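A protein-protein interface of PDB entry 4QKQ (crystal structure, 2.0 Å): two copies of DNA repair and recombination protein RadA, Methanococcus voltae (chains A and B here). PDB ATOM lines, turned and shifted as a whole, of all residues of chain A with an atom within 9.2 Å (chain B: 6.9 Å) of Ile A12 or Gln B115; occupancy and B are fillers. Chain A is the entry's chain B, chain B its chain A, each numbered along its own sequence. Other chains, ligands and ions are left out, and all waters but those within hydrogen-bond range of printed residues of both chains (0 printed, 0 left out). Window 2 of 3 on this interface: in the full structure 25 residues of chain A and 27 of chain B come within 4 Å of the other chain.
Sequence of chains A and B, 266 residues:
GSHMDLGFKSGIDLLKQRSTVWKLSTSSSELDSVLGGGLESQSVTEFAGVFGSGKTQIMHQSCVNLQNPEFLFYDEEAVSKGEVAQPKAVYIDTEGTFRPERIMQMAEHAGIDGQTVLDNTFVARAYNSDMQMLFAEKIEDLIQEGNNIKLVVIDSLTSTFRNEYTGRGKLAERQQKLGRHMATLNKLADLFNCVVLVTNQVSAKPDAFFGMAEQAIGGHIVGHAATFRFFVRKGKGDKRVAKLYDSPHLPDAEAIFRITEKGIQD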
ATOM      1  N   HIS A   3     -18.077  29.806   5.770  1.00  0.00           N
ATOM      2  CA  HIS A   3     -17.386  30.453   4.667  1.00  0.00           C
ATOM      3  C   HIS A   3     -17.899  29.975   3.310  1.00  0.00           C
ATOM      4  O   HIS A   3     -17.766  30.690   2.314  1.00  0.00           O
ATOM      5  CB  HIS A   3     -15.871  30.220   4.770  1.00  0.00           C
ATOM      6  CG  HIS A   3     -15.468  28.777   4.758  1.00  0.00           C
ATOM      7  ND1 HIS A   3     -15.519  27.977   5.880  1.00  0.00           N
ATOM      8  CD2 HIS A   3     -14.983  27.995   3.762  1.00  0.00           C
ATOM      9  CE1 HIS A   3     -15.079  26.768   5.578  1.00  0.00           C
ATOM     10  NE2 HIS A   3     -14.748  26.753   4.299  1.00  0.00           N
ATOM     11  N   MET A   4     -18.480  28.773   3.275  1.00  0.00           N
ATOM     12  CA  MET A   4     -19.025  28.211   2.037  1.00  0.00           C
ATOM     13  C   MET A   4     -20.114  29.136   1.501  1.00  0.00           C
ATOM     14  O   MET A   4     -20.257  29.304   0.287  1.00  0.00           O
ATOM     15  CB  MET A   4     -19.617  26.814   2.280  1.00  0.00           C
ATOM     16  CG  MET A   4     -18.607  25.749   2.727  1.00  0.00           C
ATOM     17  SD  MET A   4     -17.565  25.055   1.407  1.00  0.00           S
ATOM     18  CE  MET A   4     -17.901  23.312   1.586  1.00  0.00           C
ATOM     19  N   LYS A   9     -13.783  28.592  -0.385  1.00  0.00           N
ATOM     20  CA  LYS A   9     -13.634  27.161  -0.166  1.00  0.00           C
ATOM     21  C   LYS A   9     -12.215  26.973   0.359  1.00  0.00           C
ATOM     22  O   LYS A   9     -11.272  27.485  -0.238  1.00  0.00           O
ATOM     23  CB  LYS A   9     -13.736  26.359  -1.472  1.00  0.00           C
ATOM     24  CG  LYS A   9     -14.978  26.546  -2.313  1.00  0.00           C
ATOM     25  CD  LYS A   9     -14.914  25.562  -3.503  1.00  0.00           C
ATOM     26  CE  LYS A   9     -15.953  25.857  -4.591  1.00  0.00           C
ATOM     27  NZ  LYS A   9     -17.341  25.822  -4.070  1.00  0.00           N
ATOM     28  N   SER A  10     -12.038  26.233   1.442  1.00  0.00           N
ATOM     29  CA  SER A  10     -10.683  26.006   1.929  1.00  0.00           C
ATOM     30  C   SER A  10      -9.938  25.141   0.909  1.00  0.00           C
ATOM     31  O   SER A  10     -10.532  24.592  -0.031  1.00  0.00           O
ATOM     32  CB  SER A  10     -10.710  25.276   3.271  1.00  0.00           C
ATOM     33  OG  SER A  10     -11.160  23.938   3.080  1.00  0.00           O
ATOM     34  N   GLY A  11      -8.630  25.019   1.092  1.00  0.00           N
ATOM     35  CA  GLY A  11      -7.855  24.192   0.197  1.00  0.00           C
ATOM     36  C   GLY A  11      -8.333  22.749   0.327  1.00  0.00           C
ATOM     37  O   GLY A  11      -8.314  21.990  -0.647  1.00  0.00           O
ATOM     38  N   ILE A  12      -8.760  22.374   1.532  1.00  0.00           N
ATOM     39  CA  ILE A  12      -9.257  21.025   1.791  1.00  0.00           C
ATOM     40  C   ILE A  12     -10.591  20.825   1.080  1.00  0.00           C
ATOM     41  O   ILE A  12     -10.850  19.752   0.522  1.00  0.00           O
ATOM     42  CB  ILE A  12      -9.430  20.779   3.293  1.00  0.00           C
ATOM     43  CG1 ILE A  12      -8.063  20.867   3.977  1.00  0.00           C
ATOM     44  CG2 ILE A  12     -10.026  19.416   3.543  1.00  0.00           C
ATOM     45  CD1 ILE A  12      -7.032  19.896   3.396  1.00  0.00           C
ATOM     46  N   ASP A  13     -11.433  21.852   1.101  1.00  0.00           N
ATOM     47  CA  ASP A  13     -12.711  21.785   0.403  1.00  0.00           C
ATOM     48  C   ASP A  13     -12.422  21.552  -1.074  1.00  0.00           C
ATOM     49  O   ASP A  13     -13.097  20.754  -1.735  1.00  0.00           O
ATOM     50  CB  ASP A  13     -13.500  23.090   0.541  1.00  0.00           C
ATOM     51  CG  ASP A  13     -14.091  23.279   1.927  1.00  0.00           C
ATOM     52  OD1 ASP A  13     -14.393  22.258   2.586  1.00  0.00           O
ATOM     53  OD2 ASP A  13     -14.268  24.449   2.349  1.00  0.00           O
ATOM     54  N   LEU A  14     -11.414  22.244  -1.596  1.00  0.00           N
ATOM     55  CA  LEU A  14     -11.065  22.096  -3.006  1.00  0.00           C
ATOM     56  C   LEU A  14     -10.666  20.661  -3.346  1.00  0.00           C
ATOM     57  O   LEU A  14     -11.079  20.128  -4.381  1.00  0.00           O
ATOM     58  CB  LEU A  14      -9.927  23.041  -3.405  1.00  0.00           C
ATOM     59  CG  LEU A  14     -10.158  24.557  -3.470  1.00  0.00           C
ATOM     60  CD1 LEU A  14      -8.941  25.203  -4.131  1.00  0.00           C
ATOM     61  CD2 LEU A  14     -11.404  24.890  -4.271  1.00  0.00           C
ATOM     62  N   LEU A  15      -9.850  20.040  -2.497  1.00  0.00           N
ATOM     63  CA  LEU A  15      -9.442  18.666  -2.754  1.00  0.00           C
ATOM     64  C   LEU A  15     -10.651  17.733  -2.679  1.00  0.00           C
ATOM     65  O   LEU A  15     -10.839  16.878  -3.548  1.00  0.00           O
ATOM     66  CB  LEU A  15      -8.369  18.219  -1.758  1.00  0.00           C
ATOM     67  CG  LEU A  15      -6.950  18.759  -1.977  1.00  0.00           C
ATOM     68  CD1 LEU A  15      -5.968  18.054  -1.026  1.00  0.00           C
ATOM     69  CD2 LEU A  15      -6.532  18.519  -3.424  1.00  0.00           C
ATOM     70  N   LYS A  16     -11.480  17.906  -1.654  1.00  0.00           N
ATOM     71  CA  LYS A  16     -12.660  17.072  -1.486  1.00  0.00           C
ATOM     72  C   LYS A  16     -13.611  17.225  -2.662  1.00  0.00           C
ATOM     73  O   LYS A  16     -14.267  16.270  -3.070  1.00  0.00           O
ATOM     74  CB  LYS A  16     -13.352  17.408  -0.158  1.00  0.00           C
ATOM     75  CG  LYS A  16     -12.500  16.947   1.037  1.00  0.00           C
ATOM     76  CD  LYS A  16     -13.136  17.153   2.410  1.00  0.00           C
ATOM     77  CE  LYS A  16     -12.201  16.610   3.500  1.00  0.00           C
ATOM     78  NZ  LYS A  16     -12.656  16.954   4.885  1.00  0.00           N
ATOM     79  N   GLN A  17     -13.660  18.427  -3.220  1.00  0.00           N
ATOM     80  CA  GLN A  17     -14.518  18.723  -4.368  1.00  0.00           C
ATOM     81  C   GLN A  17     -14.053  17.902  -5.580  1.00  0.00           C
ATOM     82  O   GLN A  17     -14.858  17.288  -6.286  1.00  0.00           O
ATOM     83  CB  GLN A  17     -14.427  20.217  -4.684  1.00  0.00           C
ATOM     84  CG  GLN A  17     -15.436  20.736  -5.676  1.00  0.00           C
ATOM     85  CD  GLN A  17     -16.778  21.024  -5.040  1.00  0.00           C
ATOM     86  OE1 GLN A  17     -17.669  21.588  -5.676  1.00  0.00           O
ATOM     87  NE2 GLN A  17     -16.931  20.638  -3.780  1.00  0.00           N
ATOM     88  N   ARG A  18     -12.745  17.906  -5.814  1.00  0.00           N
ATOM     89  CA  ARG A  18     -12.164  17.165  -6.918  1.00  0.00           C
ATOM     90  C   ARG A  18     -12.555  15.688  -6.883  1.00  0.00           C
ATOM     91  O   ARG A  18     -12.713  15.056  -7.928  1.00  0.00           O
ATOM     92  CB  ARG A  18     -10.633  17.316  -6.908  1.00  0.00           C
ATOM     93  CG  ARG A  18     -10.135  18.461  -7.788  1.00  0.00           C
ATOM     94  CD  ARG A  18      -8.847  19.137  -7.286  1.00  0.00           C
ATOM     95  NE  ARG A  18      -7.676  18.257  -7.250  1.00  0.00           N
ATOM     96  CZ  ARG A  18      -6.414  18.691  -7.263  1.00  0.00           C
ATOM     97  NH1 ARG A  18      -6.153  19.993  -7.319  1.00  0.00           N
ATOM     98  NH2 ARG A  18      -5.408  17.826  -7.209  1.00  0.00           N
ATOM     99  N   SER A  19     -12.740  15.147  -5.684  1.00  0.00           N
ATOM    100  CA  SER A  19     -13.094  13.737  -5.537  1.00  0.00           C
ATOM    101  C   SER A  19     -14.444  13.345  -6.145  1.00  0.00           C
ATOM    102  O   SER A  19     -14.625  12.201  -6.563  1.00  0.00           O
ATOM    103  CB  SER A  19     -13.089  13.344  -4.061  1.00  0.00           C
ATOM    104  OG  SER A  19     -14.235  13.860  -3.411  1.00  0.00           O
ATOM    105  N   PRO B 100      -3.315  23.412  -5.112  1.00  0.00           N
ATOM    106  CA  PRO B 100      -3.177  22.740  -3.817  1.00  0.00           C
ATOM    107  C   PRO B 100      -1.956  21.840  -3.740  1.00  0.00           C
ATOM    108  O   PRO B 100      -1.310  21.741  -2.691  1.00  0.00           O
ATOM    109  CB  PRO B 100      -4.512  21.997  -3.654  1.00  0.00           C
ATOM    110  CG  PRO B 100      -5.115  21.990  -5.035  1.00  0.00           C
ATOM    111  CD  PRO B 100      -4.690  23.289  -5.621  1.00  0.00           C
ATOM    112  N   ILE B 103       1.012  23.787  -2.891  1.00  0.00           N
ATOM    113  CA  ILE B 103       0.972  24.093  -1.470  1.00  0.00           C
ATOM    114  C   ILE B 103       1.554  22.905  -0.681  1.00  0.00           C
ATOM    115  O   ILE B 103       2.406  23.083   0.207  1.00  0.00           O
ATOM    116  CB  ILE B 103      -0.475  24.316  -0.976  1.00  0.00           C
ATOM    117  CG1 ILE B 103      -1.072  25.600  -1.587  1.00  0.00           C
ATOM    118  CG2 ILE B 103      -0.495  24.366   0.540  1.00  0.00           C
ATOM    119  CD1 ILE B 103      -0.469  26.896  -1.074  1.00  0.00           C
ATOM    120  N   MET B 104       1.087  21.698  -1.016  1.00  0.00           N
ATOM    121  CA  MET B 104       1.537  20.481  -0.342  1.00  0.00           C
ATOM    122  C   MET B 104       3.042  20.339  -0.442  1.00  0.00           C
ATOM    123  O   MET B 104       3.719  20.079   0.553  1.00  0.00           O
ATOM    124  CB  MET B 104       0.890  19.233  -0.967  1.00  0.00           C
ATOM    125  CG  MET B 104      -0.602  19.095  -0.750  1.00  0.00           C
ATOM    126  SD  MET B 104      -1.024  19.153   0.994  1.00  0.00           S
ATOM    127  CE  MET B 104      -0.173  17.631   1.612  1.00  0.00           C
ATOM    128  N   ALA B 107       4.984  22.994   1.517  1.00  0.00           N
ATOM    129  CA  ALA B 107       4.791  22.677   2.924  1.00  0.00           C
ATOM    130  C   ALA B 107       5.694  21.528   3.350  1.00  0.00           C
ATOM    131  O   ALA B 107       6.436  21.636   4.324  1.00  0.00           O
ATOM    132  CB  ALA B 107       3.352  22.315   3.179  1.00  0.00           C
ATOM    133  N   ILE B 112       6.396  21.859   7.275  1.00  0.00           N
ATOM    134  CA  ILE B 112       5.076  22.309   7.695  1.00  0.00           C
ATOM    135  C   ILE B 112       4.033  21.304   7.190  1.00  0.00           C
ATOM    136  O   ILE B 112       4.178  20.764   6.105  1.00  0.00           O
ATOM    137  CB  ILE B 112       4.789  23.718   7.096  1.00  0.00           C
ATOM    138  CG1 ILE B 112       5.744  24.738   7.713  1.00  0.00           C
ATOM    139  CG2 ILE B 112       3.353  24.139   7.350  1.00  0.00           C
ATOM    140  CD1 ILE B 112       5.598  24.847   9.222  1.00  0.00           C
ATOM    141  N   ASP B 113       2.996  21.039   7.977  1.00  0.00           N
ATOM    142  CA  ASP B 113       1.969  20.099   7.530  1.00  0.00           C
ATOM    143  C   ASP B 113       1.119  20.741   6.434  1.00  0.00           C
ATOM    144  O   ASP B 113       0.496  21.769   6.652  1.00  0.00           O
ATOM    145  CB  ASP B 113       1.063  19.669   8.692  1.00  0.00           C
ATOM    146  CG  ASP B 113      -0.133  18.859   8.220  1.00  0.00           C
ATOM    147  OD1 ASP B 113       0.061  17.899   7.439  1.00  0.00           O
ATOM    148  OD2 ASP B 113      -1.274  19.183   8.625  1.00  0.00           O
ATOM    149  N   GLY B 114       1.099  20.117   5.264  1.00  0.00           N
ATOM    150  CA  GLY B 114       0.335  20.636   4.145  1.00  0.00           C
ATOM    151  C   GLY B 114      -1.159  20.724   4.374  1.00  0.00           C
ATOM    152  O   GLY B 114      -1.801  21.669   3.920  1.00  0.00           O
ATOM    153  N   GLN B 115      -1.725  19.743   5.068  1.00  0.00           N
ATOM    154  CA  GLN B 115      -3.158  19.758   5.332  1.00  0.00           C
ATOM    155  C   GLN B 115      -3.483  20.977   6.179  1.00  0.00           C
ATOM    156  O   GLN B 115      -4.529  21.601   6.010  1.00  0.00           O
ATOM    157  CB  GLN B 115      -3.591  18.483   6.066  1.00  0.00           C
ATOM    158  CG  GLN B 115      -4.899  17.902   5.554  1.00  0.00           C
ATOM    159  CD  GLN B 115      -4.784  17.382   4.119  1.00  0.00           C
ATOM    160  OE1 GLN B 115      -5.789  17.101   3.458  1.00  0.00           O
ATOM    161  NE2 GLN B 115      -3.554  17.248   3.636  1.00  0.00           N
ATOM    162  N   THR B 116      -2.592  21.310   7.110  1.00  0.00           N
ATOM    163  CA  THR B 116      -2.821  22.482   7.947  1.00  0.00           C
ATOM    164  C   THR B 116      -2.892  23.712   7.057  1.00  0.00           C
ATOM    165  O   THR B 116      -3.781  24.529   7.227  1.00  0.00           O
ATOM    166  CB  THR B 116      -1.712  22.664   8.997  1.00  0.00           C
ATOM    167  OG1 THR B 116      -1.767  21.566   9.923  1.00  0.00           O
ATOM    168  CG2 THR B 116      -1.901  23.969   9.756  1.00  0.00           C
ATOM    169  N   VAL B 117      -1.980  23.827   6.091  1.00  0.00           N
ATOM    170  CA  VAL B 117      -2.000  24.973   5.187  1.00  0.00           C
ATOM    171  C   VAL B 117      -3.321  25.040   4.396  1.00  0.00           C
ATOM    172  O   VAL B 117      -4.006  26.066   4.388  1.00  0.00           O
ATOM    173  CB  VAL B 117      -0.844  24.921   4.177  1.00  0.00           C
ATOM    174  CG1 VAL B 117      -0.830  26.209   3.341  1.00  0.00           C
ATOM    175  CG2 VAL B 117       0.495  24.756   4.907  1.00  0.00           C
ATOM    176  N   LEU B 118      -3.666  23.935   3.740  1.00  0.00           N
ATOM    177  CA  LEU B 118      -4.881  23.865   2.934  1.00  0.00           C
ATOM    178  C   LEU B 118      -6.129  24.108   3.765  1.00  0.00           C
ATOM    179  O   LEU B 118      -7.069  24.777   3.319  1.00  0.00           O
ATOM    180  CB  LEU B 118      -4.950  22.505   2.213  1.00  0.00           C
ATOM    181  CG  LEU B 118      -3.936  22.368   1.066  1.00  0.00           C
ATOM    182  CD1 LEU B 118      -3.980  20.975   0.466  1.00  0.00           C
ATOM    183  CD2 LEU B 118      -4.249  23.407  -0.024  1.00  0.00           C
ATOM    184  N   ASP B 119      -6.120  23.612   4.995  1.00  0.00           N
ATOM    185  CA  ASP B 119      -7.263  23.774   5.873  1.00  0.00           C
ATOM    186  C   ASP B 119      -7.417  25.212   6.369  1.00  0.00           C
ATOM    187  O   ASP B 119      -8.521  25.615   6.748  1.00  0.00           O
ATOM    188  CB  ASP B 119      -7.136  22.840   7.072  1.00  0.00           C
ATOM    189  CG  ASP B 119      -8.480  22.470   7.663  1.00  0.00           C
ATOM    190  OD1 ASP B 119      -8.535  22.208   8.882  1.00  0.00           O
ATOM    191  OD2 ASP B 119      -9.479  22.425   6.907  1.00  0.00           O
ATOM    192  N   ASN B 120      -6.323  25.977   6.372  1.00  0.00           N
ATOM    193  CA  ASN B 120      -6.364  27.377   6.832  1.00  0.00           C
ATOM    194  C   ASN B 120      -6.176  28.428   5.724  1.00  0.00           C
ATOM    195  O   ASN B 120      -5.776  29.589   5.966  1.00  0.00           O
ATOM    196  CB  ASN B 120      -5.343  27.570   7.950  1.00  0.00           C
ATOM    197  CG  ASN B 120      -5.714  26.778   9.196  1.00  0.00           C
ATOM    198  OD1 ASN B 120      -5.232  25.672   9.410  1.00  0.00           O
ATOM    199  ND2 ASN B 120      -6.608  27.323   9.993  1.00  0.00           N
ATOM    200  N   THR B 121      -6.466  28.013   4.496  1.00  0.00           N
ATOM    201  CA  THR B 121      -6.363  28.917   3.359  1.00  0.00           C
ATOM    202  C   THR B 121      -7.694  28.941   2.582  1.00  0.00           C
ATOM    203  O   THR B 121      -8.131  27.914   2.036  1.00  0.00           O
ATOM    204  CB  THR B 121      -5.215  28.499   2.438  1.00  0.00           C
ATOM    205  OG1 THR B 121      -3.970  28.606   3.155  1.00  0.00           O
ATOM    206  CG2 THR B 121      -5.165  29.391   1.198  1.00  0.00           C
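O of Thr B121 lies within hydrogen-bond range of N of Gly A11 (3.1 Å).
The backbone carbonyl oxygen (O) of Leu B118 sits at hydrogen-bond distance from the backbone NH (N) of Ile A12 (3.4 Å).
The backbone carbonyl oxygen of Leu B118 lies within hydrogen-bond range of the backbone NH of Gly A11 (2.7 Å).
The backbone carbonyl oxygen (O) of Val B117 is in hydrogen-bond range of the side-chain hydroxyl (OG1) of Thr B121, 2.8 Å away.
The backbone NH (N) of Ile A12 sits close to the side-chain hydroxyl (OG) of Ser A10 (3.3 Å).
The side-chain hydroxyl of Ser A10 is in hydrogen-bond range of the backbone NH of Asp A13 (2.9 Å).
OD1 of Asp B113 sits close to N of Gln B115, at 3.5 Å.
Among the printed residues, pairs that only touch across the chains: Lys A9 with Thr B121 (3.9 Å), Ser A10 with Leu B118 (3.7 Å), Ser A10 with Thr B121 (3.2 Å), Ile A12 with Gln B115 (3.1 Å), Ile A12 with Asp B119 (3.5 Å), Leu A15 with Leu B118 (3.8 Å) and Arg A18 with Pro B100 (3.2 Å).
Of the printed residues of chain B, Lys A9 touches Thr B121.
Printed residues of chain B within 4 Å of Ser A10: Leu B118 and Thr B121.
Of chain B, only Gln B115, Leu B118 and Asp B119 come within 4 Å of Ile A12.
Printed residues of chain B within 4 Å of Leu A15: Leu B118.
Gly B114 touches none of the printed residues of chain A.
Gln B115 touches just one residue of chain A: Ile A12.
No residue of chain A comes within 4 Å of Thr B116.
The nearest residue of chain B that does not touch Ile A12 is Gly B114 (5.5 Å).
Hydrophobic or aromatic side chains of chain B that line the printed part of chain A: Pro B100 and Leu B118.
Hydrophobic or aromatic side chains of chain A that line the printed part of chain B: Ile A12 and Leu A15.
Among the printed residues, 10 pairs touch across the chains.
No position is printed for both chains.
Of the 10 pairs that touch across the chains among the printed residues, none has its exchanged pair printed and touching as well.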
